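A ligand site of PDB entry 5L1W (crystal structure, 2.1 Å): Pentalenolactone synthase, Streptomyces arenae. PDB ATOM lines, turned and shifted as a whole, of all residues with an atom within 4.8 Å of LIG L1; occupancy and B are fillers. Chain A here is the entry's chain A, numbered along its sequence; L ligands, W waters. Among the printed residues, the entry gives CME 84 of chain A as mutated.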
ATOM      1  N   LEU A  56      15.569 -15.029  10.664  1.00  0.00           N
ATOM      2  CA  LEU A  56      14.443 -15.945  10.556  1.00  0.00           C
ATOM      3  C   LEU A  56      13.378 -15.412   9.613  1.00  0.00           C
ATOM      4  O   LEU A  56      12.644 -16.200   9.009  1.00  0.00           O
ATOM      5  CB  LEU A  56      13.844 -16.229  11.934  1.00  0.00           C
ATOM      6  CG  LEU A  56      14.634 -17.241  12.778  1.00  0.00           C
ATOM      7  CD1 LEU A  56      14.122 -17.311  14.202  1.00  0.00           C
ATOM      8  CD2 LEU A  56      14.556 -18.622  12.116  1.00  0.00           C
ATOM      9  N   CME A  84       9.794 -31.597   6.077  1.00  0.00           N
ATOM     10  CA  CME A  84       9.579 -30.153   6.078  1.00  0.00           C
ATOM     11  CB  CME A  84      10.528 -29.361   6.993  1.00  0.00           C
ATOM     12  SG  CME A  84      10.142 -29.502   8.712  1.00  0.00           S
ATOM     13  SD  CME A  84      10.816 -27.742   9.668  1.00  0.00           S
ATOM     14  CE  CME A  84      12.383 -28.103  10.402  1.00  0.00           C
ATOM     15  CZ  CME A  84      13.350 -28.827   9.490  1.00  0.00           C
ATOM     16  OH  CME A  84      14.572 -28.986  10.205  1.00  0.00           O
ATOM     17  C   CME A  84       9.637 -29.588   4.655  1.00  0.00           C
ATOM     18  O   CME A  84       9.711 -28.380   4.418  1.00  0.00           O
ATOM     19  N   HIS A  96       6.646 -26.205   0.202  1.00  0.00           N
ATOM     20  CA  HIS A  96       6.507 -25.687   1.560  1.00  0.00           C
ATOM     21  C   HIS A  96       5.267 -24.806   1.693  1.00  0.00           C
ATOM     22  O   HIS A  96       4.561 -24.876   2.704  1.00  0.00           O
ATOM     23  CB  HIS A  96       7.754 -24.910   1.984  1.00  0.00           C
ATOM     24  CG  HIS A  96       7.657 -24.347   3.363  1.00  0.00           C
ATOM     25  ND1 HIS A  96       7.830 -23.004   3.629  1.00  0.00           N
ATOM     26  CD2 HIS A  96       7.358 -24.928   4.548  1.00  0.00           C
ATOM     27  CE1 HIS A  96       7.669 -22.789   4.925  1.00  0.00           C
ATOM     28  NE2 HIS A  96       7.383 -23.943   5.499  1.00  0.00           N
ATOM     29  N   MET A  99       2.456 -27.070   2.042  1.00  0.00           N
ATOM     30  CA  MET A  99       2.488 -27.728   3.340  1.00  0.00           C
ATOM     31  C   MET A  99       1.833 -26.873   4.412  1.00  0.00           C
ATOM     32  O   MET A  99       0.945 -27.335   5.135  1.00  0.00           O
ATOM     33  CB  MET A  99       3.934 -28.059   3.736  1.00  0.00           C
ATOM     34  CG  MET A  99       4.048 -28.648   5.117  1.00  0.00           C
ATOM     35  SD  MET A  99       5.761 -28.926   5.577  1.00  0.00           S
ATOM     36  CE  MET A  99       5.531 -29.691   7.195  1.00  0.00           C
ATOM     37  N   ARG A 100       2.248 -25.604   4.509  1.00  0.00           N
ATOM     38  CA  ARG A 100       1.635 -24.712   5.491  1.00  0.00           C
ATOM     39  C   ARG A 100       0.167 -24.466   5.168  1.00  0.00           C
ATOM     40  O   ARG A 100      -0.675 -24.446   6.076  1.00  0.00           O
ATOM     41  CB  ARG A 100       2.425 -23.401   5.560  1.00  0.00           C
ATOM     42  CG  ARG A 100       3.841 -23.597   6.117  1.00  0.00           C
ATOM     43  CD  ARG A 100       4.528 -22.289   6.479  1.00  0.00           C
ATOM     44  NE  ARG A 100       3.883 -21.553   7.570  1.00  0.00           N
ATOM     45  CZ  ARG A 100       4.139 -21.746   8.865  1.00  0.00           C
ATOM     46  NH1 ARG A 100       5.018 -22.668   9.244  1.00  0.00           N
ATOM     47  NH2 ARG A 100       3.516 -21.018   9.780  1.00  0.00           N
ATOM     48  N   LEU A 103      -1.693 -27.475   6.483  1.00  0.00           N
ATOM     49  CA  LEU A 103      -1.606 -27.764   7.923  1.00  0.00           C
ATOM     50  C   LEU A 103      -2.258 -26.698   8.792  1.00  0.00           C
ATOM     51  O   LEU A 103      -2.892 -27.038   9.793  1.00  0.00           O
ATOM     52  CB  LEU A 103      -0.143 -27.949   8.344  1.00  0.00           C
ATOM     53  CG  LEU A 103       0.498 -29.261   7.883  1.00  0.00           C
ATOM     54  CD1 LEU A 103       1.948 -29.351   8.362  1.00  0.00           C
ATOM     55  CD2 LEU A 103      -0.306 -30.448   8.384  1.00  0.00           C
ATOM     56  N   PHE A 107      -5.597 -26.626  12.669  1.00  0.00           N
ATOM     57  CA  PHE A 107      -5.498 -26.209  14.067  1.00  0.00           C
ATOM     58  C   PHE A 107      -6.420 -25.008  14.300  1.00  0.00           C
ATOM     59  O   PHE A 107      -5.997 -23.974  14.816  1.00  0.00           O
ATOM     60  CB  PHE A 107      -4.035 -25.897  14.403  1.00  0.00           C
ATOM     61  CG  PHE A 107      -3.130 -27.094  14.275  1.00  0.00           C
ATOM     62  CD1 PHE A 107      -2.541 -27.411  13.062  1.00  0.00           C
ATOM     63  CD2 PHE A 107      -2.894 -27.916  15.377  1.00  0.00           C
ATOM     64  CE1 PHE A 107      -1.719 -28.532  12.940  1.00  0.00           C
ATOM     65  CE2 PHE A 107      -2.065 -29.019  15.262  1.00  0.00           C
ATOM     66  CZ  PHE A 107      -1.480 -29.331  14.042  1.00  0.00           C
ATOM     67  N   LEU A 155      -5.583 -35.670  17.524  1.00  0.00           N
ATOM     68  CA  LEU A 155      -5.394 -35.069  16.213  1.00  0.00           C
ATOM     69  C   LEU A 155      -5.561 -36.083  15.094  1.00  0.00           C
ATOM     70  O   LEU A 155      -6.163 -35.783  14.060  1.00  0.00           O
ATOM     71  CB  LEU A 155      -4.021 -34.408  16.132  1.00  0.00           C
ATOM     72  CG  LEU A 155      -3.795 -33.160  16.981  1.00  0.00           C
ATOM     73  CD1 LEU A 155      -2.354 -32.691  16.852  1.00  0.00           C
ATOM     74  CD2 LEU A 155      -4.745 -32.058  16.551  1.00  0.00           C
ATOM     75  N   VAL A 232       2.860 -34.493  11.428  1.00  0.00           N
ATOM     76  CA  VAL A 232       2.058 -34.304  12.642  1.00  0.00           C
ATOM     77  C   VAL A 232       2.499 -35.289  13.721  1.00  0.00           C
ATOM     78  O   VAL A 232       2.624 -34.919  14.900  1.00  0.00           O
ATOM     79  CB  VAL A 232       0.557 -34.437  12.330  1.00  0.00           C
ATOM     80  CG1 VAL A 232      -0.245 -34.484  13.622  1.00  0.00           C
ATOM     81  CG2 VAL A 232       0.075 -33.290  11.465  1.00  0.00           C
ATOM     82  N   PHE A 235       6.551 -34.472  14.642  1.00  0.00           N
ATOM     83  CA  PHE A 235       6.788 -33.185  15.273  1.00  0.00           C
ATOM     84  C   PHE A 235       5.781 -32.867  16.381  1.00  0.00           C
ATOM     85  O   PHE A 235       6.006 -31.919  17.145  1.00  0.00           O
ATOM     86  CB  PHE A 235       6.740 -32.045  14.233  1.00  0.00           C
ATOM     87  CG  PHE A 235       7.698 -32.203  13.075  1.00  0.00           C
ATOM     88  CD1 PHE A 235       8.857 -32.963  13.175  1.00  0.00           C
ATOM     89  CD2 PHE A 235       7.425 -31.564  11.869  1.00  0.00           C
ATOM     90  CE1 PHE A 235       9.719 -33.089  12.104  1.00  0.00           C
ATOM     91  CE2 PHE A 235       8.290 -31.686  10.785  1.00  0.00           C
ATOM     92  CZ  PHE A 235       9.437 -32.449  10.903  1.00  0.00           C
ATOM     93  N   GLY A 236       4.697 -33.629  16.488  1.00  0.00           N
ATOM     94  CA  GLY A 236       3.555 -33.230  17.287  1.00  0.00           C
ATOM     95  C   GLY A 236       3.529 -33.614  18.750  1.00  0.00           C
ATOM     96  O   GLY A 236       2.649 -33.135  19.461  1.00  0.00           O
ATOM     97  N   THR A 239       8.713 -32.859  21.125  1.00  0.00           N
ATOM     98  CA  THR A 239       9.249 -31.604  21.652  1.00  0.00           C
ATOM     99  C   THR A 239       8.410 -31.067  22.805  1.00  0.00           C
ATOM    100  O   THR A 239       8.947 -30.411  23.705  1.00  0.00           O
ATOM    101  CB  THR A 239       9.357 -30.548  20.537  1.00  0.00           C
ATOM    102  OG1 THR A 239       8.081 -30.371  19.903  1.00  0.00           O
ATOM    103  CG2 THR A 239      10.384 -30.978  19.500  1.00  0.00           C
ATOM    104  N   THR A 240       7.108 -31.330  22.801  1.00  0.00           N
ATOM    105  CA  THR A 240       6.243 -30.905  23.892  1.00  0.00           C
ATOM    106  C   THR A 240       6.555 -31.686  25.166  1.00  0.00           C
ATOM    107  O   THR A 240       6.580 -31.109  26.263  1.00  0.00           O
ATOM    108  CB  THR A 240       4.773 -31.072  23.500  1.00  0.00           C
ATOM    109  OG1 THR A 240       4.509 -30.339  22.312  1.00  0.00           O
ATOM    110  CG2 THR A 240       3.863 -30.558  24.637  1.00  0.00           C
ATOM    111  N   ARG A 243       9.453 -30.109  26.728  1.00  0.00           N
ATOM    112  CA  ARG A 243       9.149 -28.841  27.401  1.00  0.00           C
ATOM    113  C   ARG A 243       8.449 -29.040  28.732  1.00  0.00           C
ATOM    114  O   ARG A 243       8.623 -28.238  29.649  1.00  0.00           O
ATOM    115  CB  ARG A 243       8.322 -27.909  26.509  1.00  0.00           C
ATOM    116  CG  ARG A 243       9.083 -27.507  25.243  1.00  0.00           C
ATOM    117  CD  ARG A 243      10.609 -27.290  25.506  1.00  0.00           C
ATOM    118  NE  ARG A 243      11.405 -26.827  24.382  1.00  0.00           N
ATOM    119  CZ  ARG A 243      11.903 -27.640  23.450  1.00  0.00           C
ATOM    120  NH1 ARG A 243      11.601 -28.928  23.425  1.00  0.00           N
ATOM    121  NH2 ARG A 243      12.637 -27.160  22.492  1.00  0.00           N
ATOM    122  N   LEU A 276       9.390 -21.777  27.888  1.00  0.00           N
ATOM    123  CA  LEU A 276       9.786 -21.888  26.496  1.00  0.00           C
ATOM    124  C   LEU A 276      11.066 -21.113  26.226  1.00  0.00           C
ATOM    125  O   LEU A 276      11.970 -21.600  25.535  1.00  0.00           O
ATOM    126  CB  LEU A 276       8.657 -21.393  25.589  1.00  0.00           C
ATOM    127  CG  LEU A 276       7.398 -22.277  25.548  1.00  0.00           C
ATOM    128  CD1 LEU A 276       6.245 -21.537  24.887  1.00  0.00           C
ATOM    129  CD2 LEU A 276       7.699 -23.575  24.817  1.00  0.00           C
ATOM    130  N   ILE A 289      18.293 -23.389  14.849  1.00  0.00           N
ATOM    131  CA  ILE A 289      17.539 -23.566  13.611  1.00  0.00           C
ATOM    132  C   ILE A 289      18.518 -23.498  12.450  1.00  0.00           C
ATOM    133  O   ILE A 289      19.183 -22.463  12.265  1.00  0.00           O
ATOM    134  CB  ILE A 289      16.436 -22.510  13.457  1.00  0.00           C
ATOM    135  CG1 ILE A 289      15.349 -22.731  14.506  1.00  0.00           C
ATOM    136  CG2 ILE A 289      15.854 -22.574  12.057  1.00  0.00           C
ATOM    137  CD1 ILE A 289      14.226 -21.697  14.441  1.00  0.00           C
ATOM    138  N   ARG A 291      19.942 -23.348   8.503  1.00  0.00           N
ATOM    139  CA  ARG A 291      19.551 -22.703   7.258  1.00  0.00           C
ATOM    140  C   ARG A 291      20.724 -22.720   6.292  1.00  0.00           C
ATOM    141  O   ARG A 291      21.871 -22.984   6.671  1.00  0.00           O
ATOM    142  CB  ARG A 291      19.107 -21.247   7.498  1.00  0.00           C
ATOM    143  CG  ARG A 291      17.801 -21.052   8.273  1.00  0.00           C
ATOM    144  CD  ARG A 291      16.595 -21.520   7.479  1.00  0.00           C
ATOM    145  NE  ARG A 291      15.323 -21.201   8.135  1.00  0.00           N
ATOM    146  CZ  ARG A 291      14.590 -22.063   8.833  1.00  0.00           C
ATOM    147  NH1 ARG A 291      14.990 -23.324   8.988  1.00  0.00           N
ATOM    148  NH2 ARG A 291      13.452 -21.667   9.388  1.00  0.00           N
ATOM    149  N   ILE A 314      18.364 -19.946  18.514  1.00  0.00           N
ATOM    150  CA  ILE A 314      17.183 -19.413  19.187  1.00  0.00           C
ATOM    151  C   ILE A 314      17.318 -19.543  20.697  1.00  0.00           C
ATOM    152  O   ILE A 314      16.805 -18.698  21.446  1.00  0.00           O
ATOM    153  CB  ILE A 314      15.906 -20.117  18.682  1.00  0.00           C
ATOM    154  CG1 ILE A 314      16.056 -21.632  18.760  1.00  0.00           C
ATOM    155  CG2 ILE A 314      15.572 -19.651  17.271  1.00  0.00           C
ATOM    156  CD1 ILE A 314      14.790 -22.399  18.379  1.00  0.00           C
ATOM    157  N   ALA A 342      11.436 -19.477  20.694  1.00  0.00           N
ATOM    158  CA  ALA A 342      11.459 -20.924  20.861  1.00  0.00           C
ATOM    159  C   ALA A 342      10.576 -21.663  19.853  1.00  0.00           C
ATOM    160  O   ALA A 342      10.781 -22.863  19.639  1.00  0.00           O
ATOM    161  CB  ALA A 342      11.027 -21.288  22.293  1.00  0.00           C
ATOM    162  N   PHE A 343       9.588 -20.985  19.259  1.00  0.00           N
ATOM    163  CA  PHE A 343       8.791 -21.544  18.169  1.00  0.00           C
ATOM    164  C   PHE A 343       9.277 -21.057  16.805  1.00  0.00           C
ATOM    165  O   PHE A 343       8.580 -21.260  15.797  1.00  0.00           O
ATOM    166  CB  PHE A 343       7.318 -21.186  18.336  1.00  0.00           C
ATOM    167  CG  PHE A 343       6.633 -21.856  19.484  1.00  0.00           C
ATOM    168  CD1 PHE A 343       6.616 -23.235  19.613  1.00  0.00           C
ATOM    169  CD2 PHE A 343       5.949 -21.094  20.429  1.00  0.00           C
ATOM    170  CE1 PHE A 343       5.956 -23.839  20.673  1.00  0.00           C
ATOM    171  CE2 PHE A 343       5.284 -21.693  21.482  1.00  0.00           C
ATOM    172  CZ  PHE A 343       5.292 -23.070  21.611  1.00  0.00           C
ATOM    173  N   GLY A 344      10.447 -20.432  16.744  1.00  0.00           N
ATOM    174  CA  GLY A 344      10.908 -19.846  15.514  1.00  0.00           C
ATOM    175  C   GLY A 344      10.208 -18.537  15.208  1.00  0.00           C
ATOM    176  O   GLY A 344       9.640 -17.873  16.089  1.00  0.00           O
ATOM    177  N   ALA A 347       8.862 -17.578   8.009  1.00  0.00           N
ATOM    178  CA  ALA A 347       8.191 -18.465   7.064  1.00  0.00           C
ATOM    179  C   ALA A 347       7.873 -19.828   7.659  1.00  0.00           C
ATOM    180  O   ALA A 347       6.880 -20.456   7.278  1.00  0.00           O
ATOM    181  CB  ALA A 347       9.050 -18.619   5.803  1.00  0.00           C
ATOM    182  N   ARG A 348       8.694 -20.327   8.584  1.00  0.00           N
ATOM    183  CA  ARG A 348       8.492 -21.667   9.133  1.00  0.00           C
ATOM    184  C   ARG A 348       8.086 -21.647  10.600  1.00  0.00           C
ATOM    185  O   ARG A 348       8.240 -22.666  11.293  1.00  0.00           O
ATOM    186  CB  ARG A 348       9.746 -22.516   8.921  1.00  0.00           C
ATOM    187  CG  ARG A 348      10.014 -22.871   7.459  1.00  0.00           C
ATOM    188  CD  ARG A 348      11.236 -23.790   7.322  1.00  0.00           C
ATOM    189  NE  ARG A 348      11.429 -24.251   5.948  1.00  0.00           N
ATOM    190  CZ  ARG A 348      10.823 -25.303   5.425  1.00  0.00           C
ATOM    191  NH1 ARG A 348       9.981 -26.018   6.150  1.00  0.00           N
ATOM    192  NH2 ARG A 348      11.061 -25.659   4.164  1.00  0.00           N
ATOM    193  N   HIS A 349       7.571 -20.525  11.088  1.00  0.00           N
ATOM    194  CA  HIS A 349       7.016 -20.386  12.426  1.00  0.00           C
ATOM    195  C   HIS A 349       6.120 -21.573  12.778  1.00  0.00           C
ATOM    196  O   HIS A 349       5.202 -21.904  12.028  1.00  0.00           O
ATOM    197  CB  HIS A 349       6.221 -19.079  12.502  1.00  0.00           C
ATOM    198  CG  HIS A 349       6.031 -18.542  13.888  1.00  0.00           C
ATOM    199  ND1 HIS A 349       5.355 -17.365  14.142  1.00  0.00           N
ATOM    200  CD2 HIS A 349       6.443 -19.004  15.100  1.00  0.00           C
ATOM    201  CE1 HIS A 349       5.345 -17.136  15.432  1.00  0.00           C
ATOM    202  NE2 HIS A 349       5.996 -18.112  16.044  1.00  0.00           N
ATOM    203  N   CYS A 350       6.422 -22.218  13.898  1.00  0.00           N
ATOM    204  CA  CYS A 350       5.773 -23.440  14.371  1.00  0.00           C
ATOM    205  C   CYS A 350       4.265 -23.427  14.176  1.00  0.00           C
ATOM    206  O   CYS A 350       3.561 -22.526  14.643  1.00  0.00           O
ATOM    207  CB  CYS A 350       6.097 -23.633  15.855  1.00  0.00           C
ATOM    208  SG  CYS A 350       5.163 -24.968  16.631  1.00  0.00           S
ATOM    209  N   ILE A 351       3.756 -24.469  13.502  1.00  0.00           N
ATOM    210  CA  ILE A 351       2.330 -24.571  13.210  1.00  0.00           C
ATOM    211  C   ILE A 351       1.541 -25.014  14.437  1.00  0.00           C
ATOM    212  O   ILE A 351       0.378 -24.598  14.621  1.00  0.00           O
ATOM    213  CB  ILE A 351       2.118 -25.538  12.028  1.00  0.00           C
ATOM    214  CG1 ILE A 351       2.586 -24.884  10.722  1.00  0.00           C
ATOM    215  CG2 ILE A 351       0.661 -25.968  11.914  1.00  0.00           C
ATOM    216  CD1 ILE A 351       2.518 -25.791   9.516  1.00  0.00           C
ATOM    217  N   GLY A 352       2.128 -25.827  15.302  1.00  0.00           N
ATOM    218  CA  GLY A 352       1.430 -26.316  16.474  1.00  0.00           C
ATOM    219  C   GLY A 352       1.562 -25.476  17.719  1.00  0.00           C
ATOM    220  O   GLY A 352       1.148 -25.924  18.791  1.00  0.00           O
ATOM    221  N   LEU A 355      -1.475 -24.893  20.082  1.00  0.00           N
ATOM    222  CA  LEU A 355      -1.809 -26.139  20.765  1.00  0.00           C
ATOM    223  C   LEU A 355      -0.774 -26.490  21.822  1.00  0.00           C
ATOM    224  O   LEU A 355      -1.115 -26.885  22.945  1.00  0.00           O
ATOM    225  CB  LEU A 355      -1.924 -27.260  19.730  1.00  0.00           C
ATOM    226  CG  LEU A 355      -2.150 -28.669  20.271  1.00  0.00           C
ATOM    227  CD1 LEU A 355      -3.444 -28.698  21.085  1.00  0.00           C
ATOM    228  CD2 LEU A 355      -2.202 -29.669  19.125  1.00  0.00           C
ATOM    229  N   ALA A 356       0.512 -26.377  21.480  1.00  0.00           N
ATOM    230  CA  ALA A 356       1.568 -26.670  22.446  1.00  0.00           C
ATOM    231  C   ALA A 356       1.448 -25.782  23.675  1.00  0.00           C
ATOM    232  O   ALA A 356       1.599 -26.257  24.808  1.00  0.00           O
ATOM    233  CB  ALA A 356       2.938 -26.487  21.788  1.00  0.00           C
ATOM    234  N   GLU A 359      -1.294 -27.106  25.956  1.00  0.00           N
ATOM    235  CA  GLU A 359      -0.871 -28.249  26.763  1.00  0.00           C
ATOM    236  C   GLU A 359      -0.013 -27.812  27.936  1.00  0.00           C
ATOM    237  O   GLU A 359      -0.233 -28.248  29.071  1.00  0.00           O
ATOM    238  CB  GLU A 359      -0.098 -29.240  25.906  1.00  0.00           C
ATOM    239  CG  GLU A 359      -0.872 -29.831  24.742  1.00  0.00           C
ATOM    240  CD  GLU A 359      -0.052 -30.865  23.989  1.00  0.00           C
ATOM    241  OE1 GLU A 359       0.044 -30.759  22.762  1.00  0.00           O
ATOM    242  OE2 GLU A 359       0.522 -31.766  24.654  1.00  0.00           O
ATOM    243  N   LEU A 360       0.988 -26.969  27.678  1.00  0.00           N
ATOM    244  CA  LEU A 360       1.885 -26.543  28.742  1.00  0.00           C
ATOM    245  C   LEU A 360       1.142 -25.714  29.791  1.00  0.00           C
ATOM    246  O   LEU A 360       1.410 -25.848  31.000  1.00  0.00           O
ATOM    247  CB  LEU A 360       3.052 -25.762  28.152  1.00  0.00           C
ATOM    248  CG  LEU A 360       3.985 -26.576  27.237  1.00  0.00           C
ATOM    249  CD1 LEU A 360       5.084 -25.691  26.634  1.00  0.00           C
ATOM    250  CD2 LEU A 360       4.612 -27.728  27.994  1.00  0.00           C
HETATM  251  C1  LIG L   1       8.152 -25.933  13.276  1.00  0.00           C
HETATM  252  C2  LIG L   1       9.338 -25.765  17.988  1.00  0.00           C
HETATM  253  C3  LIG L   1       5.274 -28.213  19.051  1.00  0.00           C
HETATM  254  C4  LIG L   1       4.331 -28.784  14.343  1.00  0.00           C
HETATM  255  C5  LIG L   1       8.805 -25.612  14.441  1.00  0.00           C
HETATM  256  C6  LIG L   1       9.949 -24.731  14.582  1.00  0.00           C
HETATM  257  C7  LIG L   1      10.270 -24.684  15.886  1.00  0.00           C
HETATM  258  C8  LIG L   1       9.333 -25.527  16.614  1.00  0.00           C
HETATM  259  C9  LIG L   1      11.428 -23.869  16.505  1.00  0.00           C
HETATM  260  C10 LIG L   1      10.678 -23.945  13.450  1.00  0.00           C
HETATM  261  C11 LIG L   1      11.665 -24.818  12.690  1.00  0.00           C
HETATM  262  C12 LIG L   1      12.357 -24.006  11.609  1.00  0.00           C
HETATM  263  O1  LIG L   1      12.275 -22.736  11.645  1.00  0.00           O
HETATM  264  O2  LIG L   1      13.009 -24.607  10.699  1.00  0.00           O
HETATM  265  C13 LIG L   1       8.337 -26.407  18.690  1.00  0.00           C
HETATM  266  C14 LIG L   1       8.251 -26.559  20.132  1.00  0.00           C
HETATM  267  C15 LIG L   1       7.136 -27.245  20.427  1.00  0.00           C
HETATM  268  C16 LIG L   1       6.459 -27.531  19.179  1.00  0.00           C
HETATM  269  C17 LIG L   1       9.320 -26.021  21.114  1.00  0.00           C
HETATM  270  C18 LIG L   1       6.568 -27.668  21.800  1.00  0.00           C
HETATM  271  C19 LIG L   1       6.712 -26.921  22.908  1.00  0.00           C
HETATM  272  C20 LIG L   1       4.652 -28.584  17.888  1.00  0.00           C
HETATM  273  C21 LIG L   1       3.421 -29.324  17.771  1.00  0.00           C
HETATM  274  C22 LIG L   1       3.144 -29.479  16.462  1.00  0.00           C
HETATM  275  C23 LIG L   1       4.214 -28.845  15.718  1.00  0.00           C
HETATM  276  C24 LIG L   1       2.604 -29.792  18.996  1.00  0.00           C
HETATM  277  C25 LIG L   1       1.955 -30.194  15.757  1.00  0.00           C
HETATM  278  C26 LIG L   1       1.038 -30.952  16.387  1.00  0.00           C
HETATM  279  C27 LIG L   1       5.305 -28.099  13.646  1.00  0.00           C
HETATM  280  C28 LIG L   1       5.484 -28.115  12.211  1.00  0.00           C
HETATM  281  C29 LIG L   1       6.539 -27.336  11.919  1.00  0.00           C
HETATM  282  C30 LIG L   1       7.064 -26.794  13.145  1.00  0.00           C
HETATM  283  C31 LIG L   1       4.616 -28.902  11.216  1.00  0.00           C
HETATM  284  C32 LIG L   1       7.087 -27.058  10.498  1.00  0.00           C
HETATM  285  C33 LIG L   1       6.743 -25.622  10.099  1.00  0.00           C
HETATM  286  C34 LIG L   1       7.309 -25.285   8.736  1.00  0.00           C
HETATM  287  O3  LIG L   1       6.684 -24.453   8.038  1.00  0.00           O
HETATM  288  O4  LIG L   1       8.362 -25.877   8.345  1.00  0.00           O
HETATM  289  N1  LIG L   1       8.463 -26.076  15.690  1.00  0.00           N
HETATM  290  N2  LIG L   1       7.219 -27.025  18.144  1.00  0.00           N
HETATM  291  N3  LIG L   1       5.120 -28.318  16.609  1.00  0.00           N
HETATM  292  N4  LIG L   1       6.291 -27.280  14.175  1.00  0.00           N
HETATM  293 FE1  LIG L   1       6.639 -26.945  16.165  1.00  0.00          FE
HETATM  294  C1  LG2 L   2      10.919 -28.216  15.524  1.00  0.00           C
HETATM  295  C2  LG2 L   2      11.220 -29.444  14.668  1.00  0.00           C
HETATM  296  C3  LG2 L   2      10.363 -29.464  13.407  1.00  0.00           C
HETATM  297  C4  LG2 L   2      10.931 -30.746  15.435  1.00  0.00           C
HETATM  298  C5  LG2 L   2      12.415 -27.821  17.477  1.00  0.00           C
HETATM  299  C6  LG2 L   2      15.214 -29.623  16.758  1.00  0.00           C
HETATM  300  C7  LG2 L   2      14.909 -26.408  15.736  1.00  0.00           C
HETATM  301  C8  LG2 L   2      12.705 -29.199  14.282  1.00  0.00           C
HETATM  302  C9  LG2 L   2      13.470 -29.218  19.069  1.00  0.00           C
HETATM  303  C10 LG2 L   2      15.610 -28.561  14.669  1.00  0.00           C
HETATM  304  C11 LG2 L   2      13.191 -28.869  17.787  1.00  0.00           C
HETATM  305  C12 LG2 L   2      12.269 -27.656  16.077  1.00  0.00           C
HETATM  306  C13 LG2 L   2      13.696 -29.502  16.643  1.00  0.00           C
HETATM  307  C14 LG2 L   2      14.584 -27.720  15.082  1.00  0.00           C
HETATM  308  C15 LG2 L   2      13.361 -28.532  15.510  1.00  0.00           C
HETATM  309  O1  LG2 L   2      12.997 -28.548  20.009  1.00  0.00           O
HETATM  310  O2  LG2 L   2      16.181 -28.383  13.592  1.00  0.00           O
HETATM  311  O3  LG2 L   2      14.163 -30.219  19.350  1.00  0.00           O
HETATM  312  O4  LG2 L   2      15.885 -29.633  15.472  1.00  0.00           O
HETATM  313  O5  LG2 L   2      14.415 -26.500  14.349  1.00  0.00           O
HETATM  314  O   HOH W   1      14.945 -26.802  11.308  1.00  0.00           O
HETATM  315  O   HOH W   2      10.800 -20.677  12.060  1.00  0.00           O
HETATM  316  O   HOH W   3       7.915 -29.792  17.191  1.00  0.00           O
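O3 of LIG L1 lies within salt-bridge range of NH1 of Arg 100 (2.7 Å). NE2 of His 96 is in hydrogen-bond range of O3 of LIG L1 (2.7 Å). The side-chain sulfur of Cys 350 binds an iron atom (FE1) of LIG L1. NH1 of Arg 348 lies within salt-bridge range of O4 of LIG L1, at 2.7 Å. The guanidinium group of Arg 291 is in salt-bridge range of an oxygen (O1) of LIG L1, at 2.8 Å. The guanidinium group (NH2) of Arg 243 is in salt-bridge range of an oxygen (O1) of LG2 L2 (2.9 Å).
The guanidinium group (NH1) of Arg 243 is in hydrogen-bond range of the backbone carbonyl oxygen (O) of Thr 239 (3.1 Å). The backbone carbonyl oxygen (O) of Phe 343 sits at hydrogen-bond distance from the backbone NH (N) of Cys 350 (3.0 Å). The guanidinium group of Arg 100 sits close to the backbone carbonyl oxygen of Ala 347, at 3.2 Å. NH1 of Arg 348 lies within hydrogen-bond range of O of CME 84. N of Gly 352 sits close to SG of Cys 350, at 3.4 Å. A ring nitrogen (NE2) of His 96 sits close to the guanidinium group (NH1) of Arg 348 (3.4 Å). NH1 of Arg 100 is in hydrogen-bond range of O of His 349 (2.9 Å).
An oxygen (O4) of LIG L1 lies close to SD of CME 84 (3.4 Å). Residues that only touch LIG L1: Thr 239 (3.3 Å), Ala 342 (3.4 Å), Gly 236 (3.4 Å), Arg 243 (3.4 Å), Thr 240 (3.4 Å), Phe 343 (3.6 Å), Ile 289 (3.6 Å), Gly 344 (3.6 Å), Gly 352 (3.6 Å), Phe 235 (3.7 Å), Phe 107 (3.8 Å), Ala 356 (3.8 Å), Leu 155 (3.8 Å), Ile 351 (3.8 Å), Leu 103 (3.9 Å) and Leu 276 (3.98 Å). Within 4 Å of LIG L1: CME 84, His 96, Arg 100, Leu 103, Phe 107, Leu 155, Phe 235, Gly 236, Thr 239, Thr 240, Arg 243, Leu 276, Ile 289, Arg 291, Ala 342, Phe 343, Gly 344, Arg 348, Cys 350, Ile 351, Gly 352 and Ala 356. The nearest printed residue that does not touch LIG L1 is Ala 347 (4.1 Å).
Water W2 lies within hydrogen-bond range of an oxygen (O1) of LIG L1, the backbone carbonyl oxygen (O) of Arg 348 and the backbone NH (N) of His 349. Water W1 lies within hydrogen-bond range of OH of CME 84 (2.5 Å), O2 of LIG L1 (3.0 Å) and O2 of LG2 L2 (3.0 Å). Water W3 bridges OG1 of Thr 239 and O of Phe 235.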
